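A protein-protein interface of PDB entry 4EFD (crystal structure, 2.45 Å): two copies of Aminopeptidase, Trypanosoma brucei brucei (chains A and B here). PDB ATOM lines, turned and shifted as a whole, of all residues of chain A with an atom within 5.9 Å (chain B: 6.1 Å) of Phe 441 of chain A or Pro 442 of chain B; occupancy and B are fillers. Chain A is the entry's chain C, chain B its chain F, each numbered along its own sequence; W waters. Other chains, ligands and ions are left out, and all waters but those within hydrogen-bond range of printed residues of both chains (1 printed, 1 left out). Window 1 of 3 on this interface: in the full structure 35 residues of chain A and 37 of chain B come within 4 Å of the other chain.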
ATOM      1  N   ARG A 114      19.261 -26.377 -12.756  1.00  0.00           N
ATOM      2  CA  ARG A 114      18.728 -25.138 -12.193  1.00  0.00           C
ATOM      3  C   ARG A 114      17.225 -25.208 -11.907  1.00  0.00           C
ATOM      4  O   ARG A 114      16.687 -24.337 -11.223  1.00  0.00           O
ATOM      5  CB  ARG A 114      19.026 -23.963 -13.129  1.00  0.00           C
ATOM      6  CG  ARG A 114      18.624 -24.197 -14.579  1.00  0.00           C
ATOM      7  CD  ARG A 114      18.990 -23.005 -15.451  1.00  0.00           C
ATOM      8  NE  ARG A 114      18.856 -23.292 -16.876  1.00  0.00           N
ATOM      9  CZ  ARG A 114      17.745 -23.090 -17.579  1.00  0.00           C
ATOM     10  NH1 ARG A 114      17.714 -23.377 -18.873  1.00  0.00           N
ATOM     11  NH2 ARG A 114      16.665 -22.603 -16.988  1.00  0.00           N
ATOM     12  N   ASN A 115      16.557 -26.232 -12.437  1.00  0.00           N
ATOM     13  CA  ASN A 115      15.130 -26.465 -12.183  1.00  0.00           C
ATOM     14  C   ASN A 115      14.865 -27.560 -11.143  1.00  0.00           C
ATOM     15  O   ASN A 115      13.709 -27.882 -10.868  1.00  0.00           O
ATOM     16  CB  ASN A 115      14.425 -26.828 -13.491  1.00  0.00           C
ATOM     17  CG  ASN A 115      14.509 -25.724 -14.520  1.00  0.00           C
ATOM     18  OD1 ASN A 115      14.078 -24.597 -14.273  1.00  0.00           O
ATOM     19  ND2 ASN A 115      15.064 -26.040 -15.685  1.00  0.00           N
ATOM     20  N   THR A 411       5.913 -30.826 -18.946  1.00  0.00           N
ATOM     21  CA  THR A 411       6.850 -30.637 -17.832  1.00  0.00           C
ATOM     22  C   THR A 411       7.399 -31.937 -17.230  1.00  0.00           C
ATOM     23  O   THR A 411       8.435 -31.916 -16.564  1.00  0.00           O
ATOM     24  CB  THR A 411       6.214 -29.793 -16.710  1.00  0.00           C
ATOM     25  OG1 THR A 411       4.988 -30.396 -16.285  1.00  0.00           O
ATOM     26  CG2 THR A 411       5.937 -28.383 -17.203  1.00  0.00           C
ATOM     27  N   HIS A 415       7.963 -32.596 -12.352  1.00  0.00           N
ATOM     28  CA  HIS A 415       7.710 -31.156 -12.261  1.00  0.00           C
ATOM     29  C   HIS A 415       6.250 -30.820 -12.542  1.00  0.00           C
ATOM     30  O   HIS A 415       5.753 -31.073 -13.640  1.00  0.00           O
ATOM     31  CB  HIS A 415       8.594 -30.401 -13.257  1.00  0.00           C
ATOM     32  CG  HIS A 415      10.053 -30.442 -12.927  1.00  0.00           C
ATOM     33  ND1 HIS A 415      10.835 -31.555 -13.147  1.00  0.00           N
ATOM     34  CD2 HIS A 415      10.875 -29.502 -12.405  1.00  0.00           C
ATOM     35  CE1 HIS A 415      12.075 -31.300 -12.771  1.00  0.00           C
ATOM     36  NE2 HIS A 415      12.126 -30.061 -12.316  1.00  0.00           N
ATOM     37  N   ALA A 416       5.574 -30.241 -11.553  1.00  0.00           N
ATOM     38  CA  ALA A 416       4.209 -29.753 -11.737  1.00  0.00           C
ATOM     39  C   ALA A 416       4.226 -28.518 -12.630  1.00  0.00           C
ATOM     40  O   ALA A 416       5.103 -27.663 -12.495  1.00  0.00           O
ATOM     41  CB  ALA A 416       3.573 -29.423 -10.398  1.00  0.00           C
ATOM     42  N   GLY A 417       3.261 -28.433 -13.543  1.00  0.00           N
ATOM     43  CA  GLY A 417       3.164 -27.297 -14.457  1.00  0.00           C
ATOM     44  C   GLY A 417       2.563 -26.086 -13.771  1.00  0.00           C
ATOM     45  O   GLY A 417       1.570 -26.212 -13.056  1.00  0.00           O
ATOM     46  N   LEU A 418       3.160 -24.914 -13.988  1.00  0.00           N
ATOM     47  CA  LEU A 418       2.665 -23.668 -13.399  1.00  0.00           C
ATOM     48  C   LEU A 418       2.141 -22.708 -14.465  1.00  0.00           C
ATOM     49  O   LEU A 418       2.891 -22.267 -15.335  1.00  0.00           O
ATOM     50  CB  LEU A 418       3.762 -22.976 -12.580  1.00  0.00           C
ATOM     51  CG  LEU A 418       4.182 -23.651 -11.272  1.00  0.00           C
ATOM     52  CD1 LEU A 418       5.336 -22.896 -10.630  1.00  0.00           C
ATOM     53  CD2 LEU A 418       3.013 -23.756 -10.307  1.00  0.00           C
ATOM     54  N   LEU A 430       8.216 -21.380  -7.817  1.00  0.00           N
ATOM     55  CA  LEU A 430       9.338 -22.146  -8.357  1.00  0.00           C
ATOM     56  C   LEU A 430      10.449 -22.302  -7.319  1.00  0.00           C
ATOM     57  O   LEU A 430      11.021 -23.383  -7.185  1.00  0.00           O
ATOM     58  CB  LEU A 430       9.888 -21.495  -9.633  1.00  0.00           C
ATOM     59  CG  LEU A 430       9.032 -21.647 -10.895  1.00  0.00           C
ATOM     60  CD1 LEU A 430       9.598 -20.799 -12.025  1.00  0.00           C
ATOM     61  CD2 LEU A 430       8.924 -23.108 -11.319  1.00  0.00           C
ATOM     62  N   THR A 439       9.184 -30.202  -6.912  1.00  0.00           N
ATOM     63  CA  THR A 439       9.582 -29.251  -7.949  1.00  0.00           C
ATOM     64  C   THR A 439       8.483 -28.908  -8.952  1.00  0.00           C
ATOM     65  O   THR A 439       7.576 -29.703  -9.193  1.00  0.00           O
ATOM     66  CB  THR A 439      10.805 -29.777  -8.734  1.00  0.00           C
ATOM     67  OG1 THR A 439      10.592 -31.148  -9.098  1.00  0.00           O
ATOM     68  CG2 THR A 439      12.065 -29.673  -7.891  1.00  0.00           C
ATOM     69  N   CYS A 440       8.590 -27.713  -9.529  1.00  0.00           N
ATOM     70  CA  CYS A 440       7.662 -27.231 -10.549  1.00  0.00           C
ATOM     71  C   CYS A 440       8.420 -26.631 -11.733  1.00  0.00           C
ATOM     72  O   CYS A 440       9.625 -26.387 -11.654  1.00  0.00           O
ATOM     73  CB  CYS A 440       6.736 -26.167  -9.963  1.00  0.00           C
ATOM     74  SG  CYS A 440       5.657 -26.746  -8.642  1.00  0.00           S
ATOM     75  N   PHE A 441       7.700 -26.399 -12.827  1.00  0.00           N
ATOM     76  CA  PHE A 441       8.240 -25.690 -13.987  1.00  0.00           C
ATOM     77  C   PHE A 441       7.126 -24.884 -14.655  1.00  0.00           C
ATOM     78  O   PHE A 441       5.991 -25.354 -14.736  1.00  0.00           O
ATOM     79  CB  PHE A 441       8.860 -26.666 -14.987  1.00  0.00           C
ATOM     80  CG  PHE A 441       9.690 -25.996 -16.039  1.00  0.00           C
ATOM     81  CD1 PHE A 441      11.009 -25.647 -15.782  1.00  0.00           C
ATOM     82  CD2 PHE A 441       9.150 -25.689 -17.279  1.00  0.00           C
ATOM     83  CE1 PHE A 441      11.779 -25.010 -16.749  1.00  0.00           C
ATOM     84  CE2 PHE A 441       9.912 -25.057 -18.251  1.00  0.00           C
ATOM     85  CZ  PHE A 441      11.229 -24.717 -17.984  1.00  0.00           C
ATOM     86  N   PRO A 442       7.441 -23.663 -15.129  1.00  0.00           N
ATOM     87  CA  PRO A 442       6.387 -22.834 -15.712  1.00  0.00           C
ATOM     88  C   PRO A 442       5.897 -23.302 -17.081  1.00  0.00           C
ATOM     89  O   PRO A 442       6.677 -23.799 -17.896  1.00  0.00           O
ATOM     90  CB  PRO A 442       7.046 -21.457 -15.822  1.00  0.00           C
ATOM     91  CG  PRO A 442       8.485 -21.729 -15.886  1.00  0.00           C
ATOM     92  CD  PRO A 442       8.711 -22.925 -15.021  1.00  0.00           C
ATOM     93  N   VAL A 443       4.597 -23.134 -17.301  1.00  0.00           N
ATOM     94  CA  VAL A 443       3.954 -23.409 -18.578  1.00  0.00           C
ATOM     95  C   VAL A 443       3.531 -22.068 -19.194  1.00  0.00           C
ATOM     96  O   VAL A 443       3.263 -21.107 -18.468  1.00  0.00           O
ATOM     97  CB  VAL A 443       2.744 -24.342 -18.373  1.00  0.00           C
ATOM     98  CG1 VAL A 443       1.874 -24.384 -19.601  1.00  0.00           C
ATOM     99  CG2 VAL A 443       3.222 -25.741 -18.019  1.00  0.00           C
ATOM    100  N   ASN B 115       5.034 -12.937 -22.147  1.00  0.00           N
ATOM    101  CA  ASN B 115       5.725 -13.859 -23.051  1.00  0.00           C
ATOM    102  C   ASN B 115       5.521 -13.536 -24.538  1.00  0.00           C
ATOM    103  O   ASN B 115       5.965 -14.293 -25.400  1.00  0.00           O
ATOM    104  CB  ASN B 115       5.264 -15.289 -22.775  1.00  0.00           C
ATOM    105  CG  ASN B 115       5.532 -15.720 -21.350  1.00  0.00           C
ATOM    106  OD1 ASN B 115       6.667 -15.672 -20.880  1.00  0.00           O
ATOM    107  ND2 ASN B 115       4.487 -16.146 -20.655  1.00  0.00           N
ATOM    108  N   THR B 411       4.227 -25.789 -25.775  1.00  0.00           N
ATOM    109  CA  THR B 411       4.361 -24.333 -25.917  1.00  0.00           C
ATOM    110  C   THR B 411       3.417 -23.692 -26.943  1.00  0.00           C
ATOM    111  O   THR B 411       3.299 -22.468 -26.982  1.00  0.00           O
ATOM    112  CB  THR B 411       5.813 -23.938 -26.263  1.00  0.00           C
ATOM    113  OG1 THR B 411       6.200 -24.543 -27.502  1.00  0.00           O
ATOM    114  CG2 THR B 411       6.762 -24.383 -25.159  1.00  0.00           C
ATOM    115  N   ALA B 416       8.017 -21.145 -30.030  1.00  0.00           N
ATOM    116  CA  ALA B 416       8.980 -22.229 -30.201  1.00  0.00           C
ATOM    117  C   ALA B 416       9.514 -22.651 -28.837  1.00  0.00           C
ATOM    118  O   ALA B 416       9.692 -21.818 -27.950  1.00  0.00           O
ATOM    119  CB  ALA B 416      10.122 -21.794 -31.111  1.00  0.00           C
ATOM    120  N   GLY B 417       9.755 -23.947 -28.671  1.00  0.00           N
ATOM    121  CA  GLY B 417      10.258 -24.482 -27.414  1.00  0.00           C
ATOM    122  C   GLY B 417      11.762 -24.317 -27.316  1.00  0.00           C
ATOM    123  O   GLY B 417      12.480 -24.652 -28.255  1.00  0.00           O
ATOM    124  N   LEU B 418      12.232 -23.791 -26.185  1.00  0.00           N
ATOM    125  CA  LEU B 418      13.663 -23.616 -25.941  1.00  0.00           C
ATOM    126  C   LEU B 418      14.165 -24.587 -24.877  1.00  0.00           C
ATOM    127  O   LEU B 418      13.706 -24.559 -23.735  1.00  0.00           O
ATOM    128  CB  LEU B 418      13.970 -22.185 -25.500  1.00  0.00           C
ATOM    129  CG  LEU B 418      13.722 -21.078 -26.524  1.00  0.00           C
ATOM    130  CD1 LEU B 418      14.092 -19.730 -25.919  1.00  0.00           C
ATOM    131  CD2 LEU B 418      14.494 -21.319 -27.821  1.00  0.00           C
ATOM    132  N   TYR B 419      15.097 -25.448 -25.275  1.00  0.00           N
ATOM    133  CA  TYR B 419      15.814 -26.322 -24.355  1.00  0.00           C
ATOM    134  C   TYR B 419      17.270 -25.862 -24.344  1.00  0.00           C
ATOM    135  O   TYR B 419      18.001 -26.076 -25.309  1.00  0.00           O
ATOM    136  CB  TYR B 419      15.692 -27.779 -24.804  1.00  0.00           C
ATOM    137  CG  TYR B 419      16.445 -28.765 -23.942  1.00  0.00           C
ATOM    138  CD1 TYR B 419      17.734 -29.175 -24.279  1.00  0.00           C
ATOM    139  CD2 TYR B 419      15.870 -29.294 -22.792  1.00  0.00           C
ATOM    140  CE1 TYR B 419      18.431 -30.080 -23.488  1.00  0.00           C
ATOM    141  CE2 TYR B 419      16.558 -30.201 -21.997  1.00  0.00           C
ATOM    142  CZ  TYR B 419      17.835 -30.590 -22.351  1.00  0.00           C
ATOM    143  OH  TYR B 419      18.517 -31.486 -21.563  1.00  0.00           O
ATOM    144  N   GLU B 426      19.253 -18.414 -22.336  1.00  0.00           N
ATOM    145  CA  GLU B 426      17.807 -18.584 -22.481  1.00  0.00           C
ATOM    146  C   GLU B 426      17.084 -17.240 -22.459  1.00  0.00           C
ATOM    147  O   GLU B 426      16.256 -16.962 -23.328  1.00  0.00           O
ATOM    148  CB  GLU B 426      17.259 -19.479 -21.366  1.00  0.00           C
ATOM    149  CG  GLU B 426      15.834 -19.957 -21.600  1.00  0.00           C
ATOM    150  CD  GLU B 426      15.370 -20.929 -20.536  1.00  0.00           C
ATOM    151  OE1 GLU B 426      15.013 -20.479 -19.427  1.00  0.00           O
ATOM    152  OE2 GLU B 426      15.348 -22.147 -20.815  1.00  0.00           O
ATOM    153  N   LEU B 430      14.963 -15.553 -25.401  1.00  0.00           N
ATOM    154  CA  LEU B 430      13.592 -15.155 -25.071  1.00  0.00           C
ATOM    155  C   LEU B 430      13.356 -13.674 -25.365  1.00  0.00           C
ATOM    156  O   LEU B 430      12.302 -13.308 -25.886  1.00  0.00           O
ATOM    157  CB  LEU B 430      13.265 -15.455 -23.604  1.00  0.00           C
ATOM    158  CG  LEU B 430      12.950 -16.913 -23.258  1.00  0.00           C
ATOM    159  CD1 LEU B 430      12.822 -17.084 -21.752  1.00  0.00           C
ATOM    160  CD2 LEU B 430      11.683 -17.382 -23.964  1.00  0.00           C
ATOM    161  N   CYS B 440       9.307 -17.203 -28.354  1.00  0.00           N
ATOM    162  CA  CYS B 440       9.731 -18.493 -27.826  1.00  0.00           C
ATOM    163  C   CYS B 440       9.270 -18.638 -26.380  1.00  0.00           C
ATOM    164  O   CYS B 440       8.866 -17.662 -25.748  1.00  0.00           O
ATOM    165  CB  CYS B 440      11.253 -18.613 -27.887  1.00  0.00           C
ATOM    166  SG  CYS B 440      11.955 -18.652 -29.550  1.00  0.00           S
ATOM    167  N   PHE B 441       9.331 -19.861 -25.863  1.00  0.00           N
ATOM    168  CA  PHE B 441       9.053 -20.114 -24.455  1.00  0.00           C
ATOM    169  C   PHE B 441       9.882 -21.300 -23.965  1.00  0.00           C
ATOM    170  O   PHE B 441      10.035 -22.282 -24.690  1.00  0.00           O
ATOM    171  CB  PHE B 441       7.561 -20.372 -24.227  1.00  0.00           C
ATOM    172  CG  PHE B 441       7.167 -20.341 -22.781  1.00  0.00           C
ATOM    173  CD1 PHE B 441       6.989 -19.130 -22.125  1.00  0.00           C
ATOM    174  CD2 PHE B 441       7.006 -21.519 -22.065  1.00  0.00           C
ATOM    175  CE1 PHE B 441       6.647 -19.093 -20.779  1.00  0.00           C
ATOM    176  CE2 PHE B 441       6.660 -21.492 -20.722  1.00  0.00           C
ATOM    177  CZ  PHE B 441       6.482 -20.275 -20.076  1.00  0.00           C
ATOM    178  N   PRO B 442      10.424 -21.211 -22.734  1.00  0.00           N
ATOM    179  CA  PRO B 442      11.319 -22.262 -22.266  1.00  0.00           C
ATOM    180  C   PRO B 442      10.629 -23.597 -22.008  1.00  0.00           C
ATOM    181  O   PRO B 442       9.474 -23.641 -21.579  1.00  0.00           O
ATOM    182  CB  PRO B 442      11.871 -21.694 -20.954  1.00  0.00           C
ATOM    183  CG  PRO B 442      10.841 -20.749 -20.495  1.00  0.00           C
ATOM    184  CD  PRO B 442      10.313 -20.126 -21.744  1.00  0.00           C
ATOM    185  N   VAL B 443      11.361 -24.669 -22.287  1.00  0.00           N
ATOM    186  CA  VAL B 443      10.944 -26.024 -21.980  1.00  0.00           C
ATOM    187  C   VAL B 443      11.878 -26.556 -20.892  1.00  0.00           C
ATOM    188  O   VAL B 443      13.026 -26.118 -20.781  1.00  0.00           O
ATOM    189  CB  VAL B 443      10.959 -26.897 -23.266  1.00  0.00           C
ATOM    190  CG1 VAL B 443      11.421 -28.308 -22.985  1.00  0.00           C
ATOM    191  CG2 VAL B 443       9.580 -26.895 -23.922  1.00  0.00           C
ATOM    192  N   LEU B 444      11.370 -27.482 -20.084  1.00  0.00           N
ATOM    193  CA  LEU B 444      12.082 -28.005 -18.909  1.00  0.00           C
ATOM    194  C   LEU B 444      13.512 -28.465 -19.219  1.00  0.00           C
ATOM    195  O   LEU B 444      13.726 -29.285 -20.109  1.00  0.00           O
ATOM    196  CB  LEU B 444      11.267 -29.154 -18.298  1.00  0.00           C
ATOM    197  CG  LEU B 444      11.727 -29.877 -17.027  1.00  0.00           C
ATOM    198  CD1 LEU B 444      12.556 -31.104 -17.371  1.00  0.00           C
ATOM    199  CD2 LEU B 444      12.474 -28.952 -16.070  1.00  0.00           C
ATOM    200  N   TYR B 445      14.487 -27.905 -18.503  1.00  0.00           N
ATOM    201  CA  TYR B 445      15.871 -28.376 -18.574  1.00  0.00           C
ATOM    202  C   TYR B 445      16.225 -29.096 -17.275  1.00  0.00           C
ATOM    203  O   TYR B 445      16.288 -28.477 -16.209  1.00  0.00           O
ATOM    204  CB  TYR B 445      16.847 -27.222 -18.819  1.00  0.00           C
ATOM    205  CG  TYR B 445      18.290 -27.675 -18.930  1.00  0.00           C
ATOM    206  CD1 TYR B 445      18.791 -28.176 -20.127  1.00  0.00           C
ATOM    207  CD2 TYR B 445      19.150 -27.615 -17.834  1.00  0.00           C
ATOM    208  CE1 TYR B 445      20.112 -28.603 -20.235  1.00  0.00           C
ATOM    209  CE2 TYR B 445      20.473 -28.037 -17.930  1.00  0.00           C
ATOM    210  CZ  TYR B 445      20.947 -28.531 -19.133  1.00  0.00           C
ATOM    211  OH  TYR B 445      22.255 -28.949 -19.238  1.00  0.00           O
HETATM  212  O   HOH W   1       7.091 -24.997 -20.474  1.00  0.00           O
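NH1 of Arg 114 of chain A is in salt-bridge range of OE2 of Glu 426 of chain B, at 3.3 Å.
The side-chain amide nitrogen (ND2) of Asn 115 of chain A sits at hydrogen-bond distance from the backbone carbonyl oxygen (O) of Tyr 445 of chain B (2.8 Å).
The side-chain hydroxyl of Thr 411 of chain A lies within hydrogen-bond range of the backbone carbonyl oxygen of His 415 of chain A (2.8 Å).
The backbone NH (N) of Phe 441 of chain A sits at hydrogen-bond distance from the backbone carbonyl oxygen (O) of Ala 416 of chain A (2.9 Å).
N of Leu 418 of chain A lies within hydrogen-bond range of O of Phe 441 of chain A (3.0 Å).
O of Leu 418 of chain A is in hydrogen-bond range of N of Val 443 of chain A, 2.7 Å away.
The backbone carbonyl oxygen (O) of Phe 441 of chain B sits at hydrogen-bond distance from the backbone NH (N) of Leu 418 of chain B, at 3.1 Å.
O of Leu 418 of chain B lies within hydrogen-bond range of N of Val 443 of chain B (2.8 Å).
Among the printed residues, pairs that only touch across the chains: Arg 114 of chain A with Tyr 445 of chain B, Asn 115 of chain A with Leu 444 of chain B, Thr 411 of chain A with Leu 444 of chain B, His 415 of chain A with Leu 444 of chain B, Phe 441 of chain A with Pro 442 of chain B, Phe 441 of chain A with Val 443 of chain B, Phe 441 of chain A with Leu 444 of chain B, Pro 442 of chain A with Phe 441 of chain B and Val 443 of chain A with Phe 441 of chain B.
Of the printed residues of chain B, Thr 411 of chain A touches Leu 444.
Phe 441 of chain A touches three residues of chain B.
Of the printed residues of chain B, Val 443 of chain A touches Phe 441.
Ala 416 of chain B touches none of the printed residues of chain A.
Of the printed residues of chain A, Glu 426 of chain B touches Arg 114 (3.3 Å).
Of the printed residues of chain A, Phe 441 of chain B touches Pro 442 (3.6 Å) and Val 443 (3.5 Å).
The nearest printed residue of chain A that does not touch Glu 426 of chain B is Phe 441 of chain A (5.6 Å).
Printed residues of chain A that touch a printed residue of chain B: Arg 114, Asn 115, Thr 411, His 415, Phe 441, Pro 442 and Val 443.
Hydrophobic or aromatic side chains of chain A within 4 Å of the printed part of chain B: His 415 and Phe 441.
Along chain A the printed residues that touch a printed residue of chain B span positions 114 to 443.
Among the printed residues, 11 pairs touch across the chains.
Phe 441 of chain A touches Pro 442 of chain B, and with the chains exchanged Pro 442 of chain A touches Phe 441 of chain B.
Phe 441 of chain A touches Val 443 of chain B, and with the chains exchanged Val 443 of chain A touches Phe 441 of chain B.
Of the 11 pairs that touch across the chains among the printed residues, 4 have their exchanged pair printed and touching as well.
Water W1 bridges the backbone carbonyl oxygen of Pro 442 of chain A (2.9 Å) and the backbone carbonyl oxygen of Pro 442 of chain B (3.0 Å).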
